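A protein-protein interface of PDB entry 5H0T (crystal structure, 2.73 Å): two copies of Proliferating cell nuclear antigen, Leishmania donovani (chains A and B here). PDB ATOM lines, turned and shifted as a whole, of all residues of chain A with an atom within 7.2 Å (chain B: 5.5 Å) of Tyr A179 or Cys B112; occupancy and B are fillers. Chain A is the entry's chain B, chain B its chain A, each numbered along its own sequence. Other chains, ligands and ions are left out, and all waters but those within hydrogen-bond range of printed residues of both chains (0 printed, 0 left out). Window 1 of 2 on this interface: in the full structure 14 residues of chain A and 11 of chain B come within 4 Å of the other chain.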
ATOM      1  N   GLU A 143      14.558  -6.349  13.529  1.00  0.00           N
ATOM      2  CA  GLU A 143      13.351  -6.623  14.336  1.00  0.00           C
ATOM      3  C   GLU A 143      12.279  -5.639  13.941  1.00  0.00           C
ATOM      4  O   GLU A 143      11.125  -6.005  13.696  1.00  0.00           O
ATOM      5  CB  GLU A 143      13.643  -6.557  15.861  1.00  0.00           C
ATOM      6  CG  GLU A 143      12.503  -6.979  16.814  1.00  0.00           C
ATOM      7  CD  GLU A 143      11.974  -8.404  16.581  1.00  0.00           C
ATOM      8  OE1 GLU A 143      12.771  -9.294  16.245  1.00  0.00           O
ATOM      9  OE2 GLU A 143      10.753  -8.657  16.695  1.00  0.00           O
ATOM     10  N   ILE A 147       8.716  -6.585  12.498  1.00  0.00           N
ATOM     11  CA  ILE A 147       7.492  -6.084  13.106  1.00  0.00           C
ATOM     12  C   ILE A 147       6.555  -5.351  12.120  1.00  0.00           C
ATOM     13  O   ILE A 147       5.349  -5.559  12.172  1.00  0.00           O
ATOM     14  CB  ILE A 147       7.793  -5.167  14.293  1.00  0.00           C
ATOM     15  CG1 ILE A 147       8.389  -5.985  15.434  1.00  0.00           C
ATOM     16  CG2 ILE A 147       6.526  -4.488  14.808  1.00  0.00           C
ATOM     17  CD1 ILE A 147       9.020  -5.129  16.505  1.00  0.00           C
ATOM     18  N   ASP A 150       4.982  -7.835   9.762  1.00  0.00           N
ATOM     19  CA  ASP A 150       4.052  -8.593  10.546  1.00  0.00           C
ATOM     20  C   ASP A 150       2.778  -7.837  10.725  1.00  0.00           C
ATOM     21  O   ASP A 150       1.728  -8.350  10.384  1.00  0.00           O
ATOM     22  CB  ASP A 150       4.640  -8.938  11.937  1.00  0.00           C
ATOM     23  CG  ASP A 150       5.782  -9.988  11.881  1.00  0.00           C
ATOM     24  OD1 ASP A 150       6.183 -10.494  10.746  1.00  0.00           O
ATOM     25  OD2 ASP A 150       6.249 -10.309  13.021  1.00  0.00           O
ATOM     26  N   MET A 151       2.861  -6.609  11.244  1.00  0.00           N
ATOM     27  CA  MET A 151       1.658  -5.797  11.496  1.00  0.00           C
ATOM     28  C   MET A 151       0.818  -5.610  10.243  1.00  0.00           C
ATOM     29  O   MET A 151      -0.394  -5.474  10.333  1.00  0.00           O
ATOM     30  CB  MET A 151       2.023  -4.447  12.083  1.00  0.00           C
ATOM     31  CG  MET A 151       2.562  -4.469  13.505  1.00  0.00           C
ATOM     32  SD  MET A 151       1.508  -5.199  14.737  1.00  0.00           S
ATOM     33  CE  MET A 151       2.135  -6.897  14.729  1.00  0.00           C
ATOM     34  N   PHE A 154      -2.472  -7.662   9.529  1.00  0.00           N
ATOM     35  CA  PHE A 154      -3.713  -7.200  10.141  1.00  0.00           C
ATOM     36  C   PHE A 154      -4.288  -6.006   9.436  1.00  0.00           C
ATOM     37  O   PHE A 154      -5.359  -6.098   8.884  1.00  0.00           O
ATOM     38  CB  PHE A 154      -3.513  -6.962  11.619  1.00  0.00           C
ATOM     39  CG  PHE A 154      -3.032  -8.174  12.316  1.00  0.00           C
ATOM     40  CD1 PHE A 154      -3.909  -9.193  12.663  1.00  0.00           C
ATOM     41  CD2 PHE A 154      -1.687  -8.363  12.512  1.00  0.00           C
ATOM     42  CE1 PHE A 154      -3.454 -10.343  13.246  1.00  0.00           C
ATOM     43  CE2 PHE A 154      -1.212  -9.512  13.104  1.00  0.00           C
ATOM     44  CZ  PHE A 154      -2.102 -10.503  13.482  1.00  0.00           C
ATOM     45  N   THR A 159      -0.192   1.218  15.465  1.00  0.00           N
ATOM     46  CA  THR A 159      -0.143   2.104  16.604  1.00  0.00           C
ATOM     47  C   THR A 159       1.026   1.756  17.478  1.00  0.00           C
ATOM     48  O   THR A 159       1.067   0.682  18.063  1.00  0.00           O
ATOM     49  CB  THR A 159      -1.394   1.956  17.464  1.00  0.00           C
ATOM     50  OG1 THR A 159      -2.515   2.283  16.668  1.00  0.00           O
ATOM     51  CG2 THR A 159      -1.337   2.871  18.661  1.00  0.00           C
ATOM     52  N   VAL A 167       8.059  -0.551  24.184  1.00  0.00           N
ATOM     53  CA  VAL A 167       7.213  -0.083  23.104  1.00  0.00           C
ATOM     54  C   VAL A 167       6.297  -1.220  22.609  1.00  0.00           C
ATOM     55  O   VAL A 167       6.680  -2.387  22.538  1.00  0.00           O
ATOM     56  CB  VAL A 167       8.008   0.452  21.912  1.00  0.00           C
ATOM     57  CG1 VAL A 167       8.448   1.897  21.951  1.00  0.00           C
ATOM     58  CG2 VAL A 167       9.010  -0.575  21.514  1.00  0.00           C
ATOM     59  N   LYS A 168       5.039  -0.863  22.335  1.00  0.00           N
ATOM     60  CA  LYS A 168       4.018  -1.760  21.840  1.00  0.00           C
ATOM     61  C   LYS A 168       3.508  -1.329  20.471  1.00  0.00           C
ATOM     62  O   LYS A 168       2.861  -0.292  20.345  1.00  0.00           O
ATOM     63  CB  LYS A 168       2.850  -1.815  22.826  1.00  0.00           C
ATOM     64  CG  LYS A 168       1.717  -2.731  22.398  1.00  0.00           C
ATOM     65  CD  LYS A 168       0.893  -3.248  23.591  1.00  0.00           C
ATOM     66  CE  LYS A 168      -0.586  -3.115  23.301  1.00  0.00           C
ATOM     67  NZ  LYS A 168      -1.352  -3.987  24.234  1.00  0.00           N
ATOM     68  N   PHE A 169       3.765  -2.172  19.475  1.00  0.00           N
ATOM     69  CA  PHE A 169       3.232  -2.027  18.130  1.00  0.00           C
ATOM     70  C   PHE A 169       1.926  -2.843  17.973  1.00  0.00           C
ATOM     71  O   PHE A 169       1.927  -4.002  18.273  1.00  0.00           O
ATOM     72  CB  PHE A 169       4.248  -2.541  17.144  1.00  0.00           C
ATOM     73  CG  PHE A 169       5.573  -1.884  17.231  1.00  0.00           C
ATOM     74  CD1 PHE A 169       6.546  -2.376  18.074  1.00  0.00           C
ATOM     75  CD2 PHE A 169       5.882  -0.837  16.407  1.00  0.00           C
ATOM     76  CE1 PHE A 169       7.813  -1.791  18.129  1.00  0.00           C
ATOM     77  CE2 PHE A 169       7.146  -0.261  16.427  1.00  0.00           C
ATOM     78  CZ  PHE A 169       8.109  -0.740  17.291  1.00  0.00           C
ATOM     79  N   SER A 170       0.847  -2.233  17.479  1.00  0.00           N
ATOM     80  CA  SER A 170      -0.505  -2.839  17.446  1.00  0.00           C
ATOM     81  C   SER A 170      -1.159  -2.576  16.099  1.00  0.00           C
ATOM     82  O   SER A 170      -0.981  -1.516  15.527  1.00  0.00           O
ATOM     83  CB  SER A 170      -1.409  -2.229  18.511  1.00  0.00           C
ATOM     84  OG  SER A 170      -0.634  -1.724  19.588  1.00  0.00           O
ATOM     85  N   SER A 171      -1.945  -3.532  15.617  1.00  0.00           N
ATOM     86  CA  SER A 171      -2.650  -3.382  14.353  1.00  0.00           C
ATOM     87  C   SER A 171      -3.942  -4.179  14.386  1.00  0.00           C
ATOM     88  O   SER A 171      -4.058  -5.089  15.196  1.00  0.00           O
ATOM     89  CB  SER A 171      -1.756  -3.825  13.213  1.00  0.00           C
ATOM     90  OG  SER A 171      -2.203  -3.265  11.989  1.00  0.00           O
ATOM     91  N   GLN A 177      -6.489  -9.112  15.310  1.00  0.00           N
ATOM     92  CA  GLN A 177      -5.756  -8.061  16.022  1.00  0.00           C
ATOM     93  C   GLN A 177      -4.430  -8.618  16.443  1.00  0.00           C
ATOM     94  O   GLN A 177      -4.354  -9.742  16.889  1.00  0.00           O
ATOM     95  CB  GLN A 177      -6.480  -7.680  17.282  1.00  0.00           C
ATOM     96  CG  GLN A 177      -7.930  -7.259  17.123  1.00  0.00           C
ATOM     97  CD  GLN A 177      -8.622  -7.306  18.461  1.00  0.00           C
ATOM     98  OE1 GLN A 177      -8.013  -6.912  19.444  1.00  0.00           O
ATOM     99  NE2 GLN A 177      -9.855  -7.854  18.527  1.00  0.00           N
ATOM    100  N   GLY A 178      -3.375  -7.832  16.323  1.00  0.00           N
ATOM    101  CA  GLY A 178      -2.053  -8.273  16.725  1.00  0.00           C
ATOM    102  C   GLY A 178      -1.344  -7.220  17.551  1.00  0.00           C
ATOM    103  O   GLY A 178      -1.621  -6.045  17.431  1.00  0.00           O
ATOM    104  N   TYR A 179      -0.419  -7.654  18.381  1.00  0.00           N
ATOM    105  CA  TYR A 179       0.606  -6.763  18.872  1.00  0.00           C
ATOM    106  C   TYR A 179       1.927  -7.448  19.086  1.00  0.00           C
ATOM    107  O   TYR A 179       2.004  -8.654  19.210  1.00  0.00           O
ATOM    108  CB  TYR A 179       0.144  -5.993  20.120  1.00  0.00           C
ATOM    109  CG  TYR A 179       0.217  -6.700  21.453  1.00  0.00           C
ATOM    110  CD1 TYR A 179       1.430  -6.946  22.080  1.00  0.00           C
ATOM    111  CD2 TYR A 179      -0.956  -7.054  22.127  1.00  0.00           C
ATOM    112  CE1 TYR A 179       1.476  -7.591  23.316  1.00  0.00           C
ATOM    113  CE2 TYR A 179      -0.918  -7.697  23.343  1.00  0.00           C
ATOM    114  CZ  TYR A 179       0.303  -7.956  23.944  1.00  0.00           C
ATOM    115  OH  TYR A 179       0.324  -8.613  25.163  1.00  0.00           O
ATOM    116  N   THR A 180       2.965  -6.644  19.092  1.00  0.00           N
ATOM    117  CA  THR A 180       4.307  -7.059  19.461  1.00  0.00           C
ATOM    118  C   THR A 180       4.740  -6.067  20.509  1.00  0.00           C
ATOM    119  O   THR A 180       4.646  -4.876  20.299  1.00  0.00           O
ATOM    120  CB  THR A 180       5.247  -7.027  18.245  1.00  0.00           C
ATOM    121  OG1 THR A 180       4.788  -7.982  17.299  1.00  0.00           O
ATOM    122  CG2 THR A 180       6.631  -7.406  18.622  1.00  0.00           C
ATOM    123  N   PHE A 181       5.148  -6.577  21.653  1.00  0.00           N
ATOM    124  CA  PHE A 181       5.634  -5.744  22.730  1.00  0.00           C
ATOM    125  C   PHE A 181       7.099  -6.071  22.920  1.00  0.00           C
ATOM    126  O   PHE A 181       7.479  -7.227  23.060  1.00  0.00           O
ATOM    127  CB  PHE A 181       4.826  -5.976  23.996  1.00  0.00           C
ATOM    128  CG  PHE A 181       5.329  -5.211  25.179  1.00  0.00           C
ATOM    129  CD1 PHE A 181       6.394  -5.687  25.925  1.00  0.00           C
ATOM    130  CD2 PHE A 181       4.722  -4.006  25.559  1.00  0.00           C
ATOM    131  CE1 PHE A 181       6.867  -4.971  27.003  1.00  0.00           C
ATOM    132  CE2 PHE A 181       5.184  -3.296  26.645  1.00  0.00           C
ATOM    133  CZ  PHE A 181       6.273  -3.770  27.356  1.00  0.00           C
ATOM    134  N   LEU A 182       7.922  -5.031  22.879  1.00  0.00           N
ATOM    135  CA  LEU A 182       9.340  -5.141  23.143  1.00  0.00           C
ATOM    136  C   LEU A 182       9.611  -4.468  24.467  1.00  0.00           C
ATOM    137  O   LEU A 182       9.146  -3.360  24.711  1.00  0.00           O
ATOM    138  CB  LEU A 182      10.133  -4.463  22.057  1.00  0.00           C
ATOM    139  CG  LEU A 182       9.982  -5.040  20.662  1.00  0.00           C
ATOM    140  CD1 LEU A 182      10.785  -4.208  19.671  1.00  0.00           C
ATOM    141  CD2 LEU A 182      10.393  -6.498  20.572  1.00  0.00           C
ATOM    142  N   LEU B 101      -3.496 -16.192  20.639  1.00  0.00           N
ATOM    143  CA  LEU B 101      -2.213 -16.825  20.461  1.00  0.00           C
ATOM    144  C   LEU B 101      -1.175 -15.920  21.027  1.00  0.00           C
ATOM    145  O   LEU B 101      -1.165 -14.750  20.731  1.00  0.00           O
ATOM    146  CB  LEU B 101      -1.966 -17.050  18.965  1.00  0.00           C
ATOM    147  CG  LEU B 101      -2.910 -18.086  18.399  1.00  0.00           C
ATOM    148  CD1 LEU B 101      -2.952 -17.933  16.934  1.00  0.00           C
ATOM    149  CD2 LEU B 101      -2.375 -19.458  18.704  1.00  0.00           C
ATOM    150  N   THR B 102      -0.296 -16.452  21.860  1.00  0.00           N
ATOM    151  CA  THR B 102       0.705 -15.646  22.557  1.00  0.00           C
ATOM    152  C   THR B 102       2.067 -16.282  22.375  1.00  0.00           C
ATOM    153  O   THR B 102       2.297 -17.435  22.718  1.00  0.00           O
ATOM    154  CB  THR B 102       0.358 -15.446  24.023  1.00  0.00           C
ATOM    155  OG1 THR B 102      -0.956 -14.842  24.132  1.00  0.00           O
ATOM    156  CG2 THR B 102       1.358 -14.518  24.670  1.00  0.00           C
ATOM    157  N   SER B 103       2.969 -15.495  21.805  1.00  0.00           N
ATOM    158  CA  SER B 103       4.291 -15.942  21.477  1.00  0.00           C
ATOM    159  C   SER B 103       5.246 -15.201  22.374  1.00  0.00           C
ATOM    160  O   SER B 103       5.004 -14.050  22.742  1.00  0.00           O
ATOM    161  CB  SER B 103       4.602 -15.645  20.013  1.00  0.00           C
ATOM    162  OG  SER B 103       5.931 -15.174  19.850  1.00  0.00           O
ATOM    163  N   GLU B 104       6.320 -15.885  22.753  1.00  0.00           N
ATOM    164  CA  GLU B 104       7.374 -15.275  23.530  1.00  0.00           C
ATOM    165  C   GLU B 104       8.678 -15.875  23.093  1.00  0.00           C
ATOM    166  O   GLU B 104       8.757 -17.052  22.764  1.00  0.00           O
ATOM    167  CB  GLU B 104       7.150 -15.493  25.025  1.00  0.00           C
ATOM    168  CG  GLU B 104       7.309 -14.248  25.901  1.00  0.00           C
ATOM    169  CD  GLU B 104       6.430 -14.357  27.166  1.00  0.00           C
ATOM    170  OE1 GLU B 104       5.557 -13.494  27.512  1.00  0.00           O
ATOM    171  OE2 GLU B 104       6.624 -15.379  27.850  1.00  0.00           O
ATOM    172  N   ARG B 110      10.653 -10.194  24.132  1.00  0.00           N
ATOM    173  CA  ARG B 110       9.616  -9.914  23.149  1.00  0.00           C
ATOM    174  C   ARG B 110       8.408 -10.812  23.409  1.00  0.00           C
ATOM    175  O   ARG B 110       8.544 -11.992  23.599  1.00  0.00           O
ATOM    176  CB  ARG B 110      10.119 -10.158  21.709  1.00  0.00           C
ATOM    177  CG  ARG B 110       9.014  -9.984  20.660  1.00  0.00           C
ATOM    178  CD  ARG B 110       9.448 -10.138  19.212  1.00  0.00           C
ATOM    179  NE  ARG B 110       9.652 -11.541  18.864  1.00  0.00           N
ATOM    180  CZ  ARG B 110      10.801 -12.101  18.487  1.00  0.00           C
ATOM    181  NH1 ARG B 110      11.914 -11.385  18.368  1.00  0.00           N
ATOM    182  NH2 ARG B 110      10.846 -13.405  18.213  1.00  0.00           N
ATOM    183  N   LYS B 111       7.234 -10.213  23.370  1.00  0.00           N
ATOM    184  CA  LYS B 111       5.967 -10.866  23.540  1.00  0.00           C
ATOM    185  C   LYS B 111       5.043 -10.386  22.435  1.00  0.00           C
ATOM    186  O   LYS B 111       4.893  -9.189  22.205  1.00  0.00           O
ATOM    187  CB  LYS B 111       5.370 -10.526  24.915  1.00  0.00           C
ATOM    188  CG  LYS B 111       3.857 -10.756  25.117  1.00  0.00           C
ATOM    189  CD  LYS B 111       3.522 -11.080  26.571  1.00  0.00           C
ATOM    190  CE  LYS B 111       2.252 -10.428  27.081  1.00  0.00           C
ATOM    191  NZ  LYS B 111       1.141 -11.371  27.408  1.00  0.00           N
ATOM    192  N   CYS B 112       4.410 -11.334  21.766  1.00  0.00           N
ATOM    193  CA  CYS B 112       3.456 -11.055  20.721  1.00  0.00           C
ATOM    194  C   CYS B 112       2.170 -11.668  21.142  1.00  0.00           C
ATOM    195  O   CYS B 112       2.183 -12.744  21.712  1.00  0.00           O
ATOM    196  CB  CYS B 112       3.906 -11.685  19.413  1.00  0.00           C
ATOM    197  SG  CYS B 112       5.506 -11.086  18.904  1.00  0.00           S
ATOM    198  N   GLU B 113       1.052 -11.008  20.835  1.00  0.00           N
ATOM    199  CA  GLU B 113      -0.250 -11.582  21.087  1.00  0.00           C
ATOM    200  C   GLU B 113      -1.225 -11.259  19.961  1.00  0.00           C
ATOM    201  O   GLU B 113      -1.448 -10.115  19.608  1.00  0.00           O
ATOM    202  CB  GLU B 113      -0.789 -11.086  22.415  1.00  0.00           C
ATOM    203  CG  GLU B 113      -2.051 -11.771  22.902  1.00  0.00           C
ATOM    204  CD  GLU B 113      -2.581 -11.147  24.156  1.00  0.00           C
ATOM    205  OE1 GLU B 113      -2.028 -11.492  25.239  1.00  0.00           O
ATOM    206  OE2 GLU B 113      -3.518 -10.297  24.011  1.00  0.00           O
ATOM    207  N   TYR B 114      -1.845 -12.303  19.439  1.00  0.00           N
ATOM    208  CA  TYR B 114      -2.745 -12.238  18.323  1.00  0.00           C
ATOM    209  C   TYR B 114      -4.087 -12.770  18.782  1.00  0.00           C
ATOM    210  O   TYR B 114      -4.129 -13.619  19.648  1.00  0.00           O
ATOM    211  CB  TYR B 114      -2.171 -13.112  17.191  1.00  0.00           C
ATOM    212  CG  TYR B 114      -0.732 -12.744  16.865  1.00  0.00           C
ATOM    213  CD1 TYR B 114      -0.435 -11.495  16.354  1.00  0.00           C
ATOM    214  CD2 TYR B 114       0.315 -13.618  17.089  1.00  0.00           C
ATOM    215  CE1 TYR B 114       0.865 -11.130  16.024  1.00  0.00           C
ATOM    216  CE2 TYR B 114       1.625 -13.267  16.762  1.00  0.00           C
ATOM    217  CZ  TYR B 114       1.903 -12.018  16.238  1.00  0.00           C
ATOM    218  OH  TYR B 114       3.195 -11.609  15.940  1.00  0.00           O
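The guanidinium group (NH1) of Arg B110 lies within salt-bridge range of the side-chain carboxylate (OE1) of Glu A143, at 3.1 Å.
The backbone carbonyl oxygen of Lys B111 sits at hydrogen-bond distance from the backbone NH of Phe A181 (2.7 Å).
The side-chain hydroxyl (OG1) of Thr A180 sits at hydrogen-bond distance from the side-chain sulfur (SG) of Cys B112.
The backbone carbonyl oxygen (O) of Glu B113 sits at hydrogen-bond distance from the backbone NH (N) of Tyr A179 (2.9 Å).
The backbone carbonyl oxygen of Tyr B114 is in hydrogen-bond range of the backbone NH of Leu B101 (2.8 Å).
The backbone NH of Ser B103 sits at hydrogen-bond distance from the backbone carbonyl oxygen of Cys B112 (2.9 Å).
NZ of Lys B111 lies within salt-bridge range of OE1 of Glu B113.
OH of Tyr B114 sits close to SG of Cys B112.
The backbone carbonyl oxygen of Val A167 lies within hydrogen-bond range of the backbone NH of Leu A182 (2.9 Å).
The backbone carbonyl oxygen (O) of Ser A171 sits at hydrogen-bond distance from the backbone NH (N) of Gly A178.
Among the printed residues, merely in contact across the chains: Phe A154 with Tyr B114 (3.5 Å), Gln A177 with Glu B113 (3.997 Å), Gln A177 with Tyr B114 (3.3 Å), Gly A178 with Glu B113 (3.5 Å), Gly A178 with Tyr B114 (3.6 Å), Tyr A179 with Lys B111 (3.3 Å), Tyr A179 with Cys B112 (3.2 Å), Thr A180 with Arg B110 (3.97 Å), Thr A180 with Lys B111 (3.5 Å), Phe A181 with Arg B110 (3.4 Å) and Leu A182 with Arg B110 (3.7 Å).
Tyr A179 touches just these residues of chain B: Lys B111, Cys B112 and Glu B113.
Cys B112 touches just these residues of chain A: Tyr A179 and Thr A180.
Of the printed residues of chain A, Glu B113 touches Gln A177 (3.997 Å), Gly A178 (3.5 Å) and Tyr A179 (2.9 Å).
Of the printed residues of chain B, Gln A177 touches Glu B113 (3.997 Å) and Tyr B114 (3.3 Å).
Printed residues of chain B within 4 Å of Leu A182: Arg B110.
Of the printed residues of chain B, Phe A181 touches Arg B110 and Lys B111.
Thr B102 touches none of the printed residues of chain A.
Phe A169 touches none of the printed residues of chain B.
The nearest printed residue of chain B that does not touch Glu A143 is Cys B112 (6.2 Å).
Hydrophobic or aromatic side chains of chain A that line the printed part of chain B: Phe A154, Tyr A179, Phe A181 and Leu A182.
Hydrophobic or aromatic side chains of chain B within 4 Å of the printed part of chain A: Tyr B114.
Among the printed residues, 15 pairs touch across the chains.
Among the printed residues, Asp or Glu carboxylates within 4 Å of a Lys or Arg side-chain nitrogen of the other chain: Glu A143 with Arg B110 (3.1 Å).
No position is printed for both chains.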
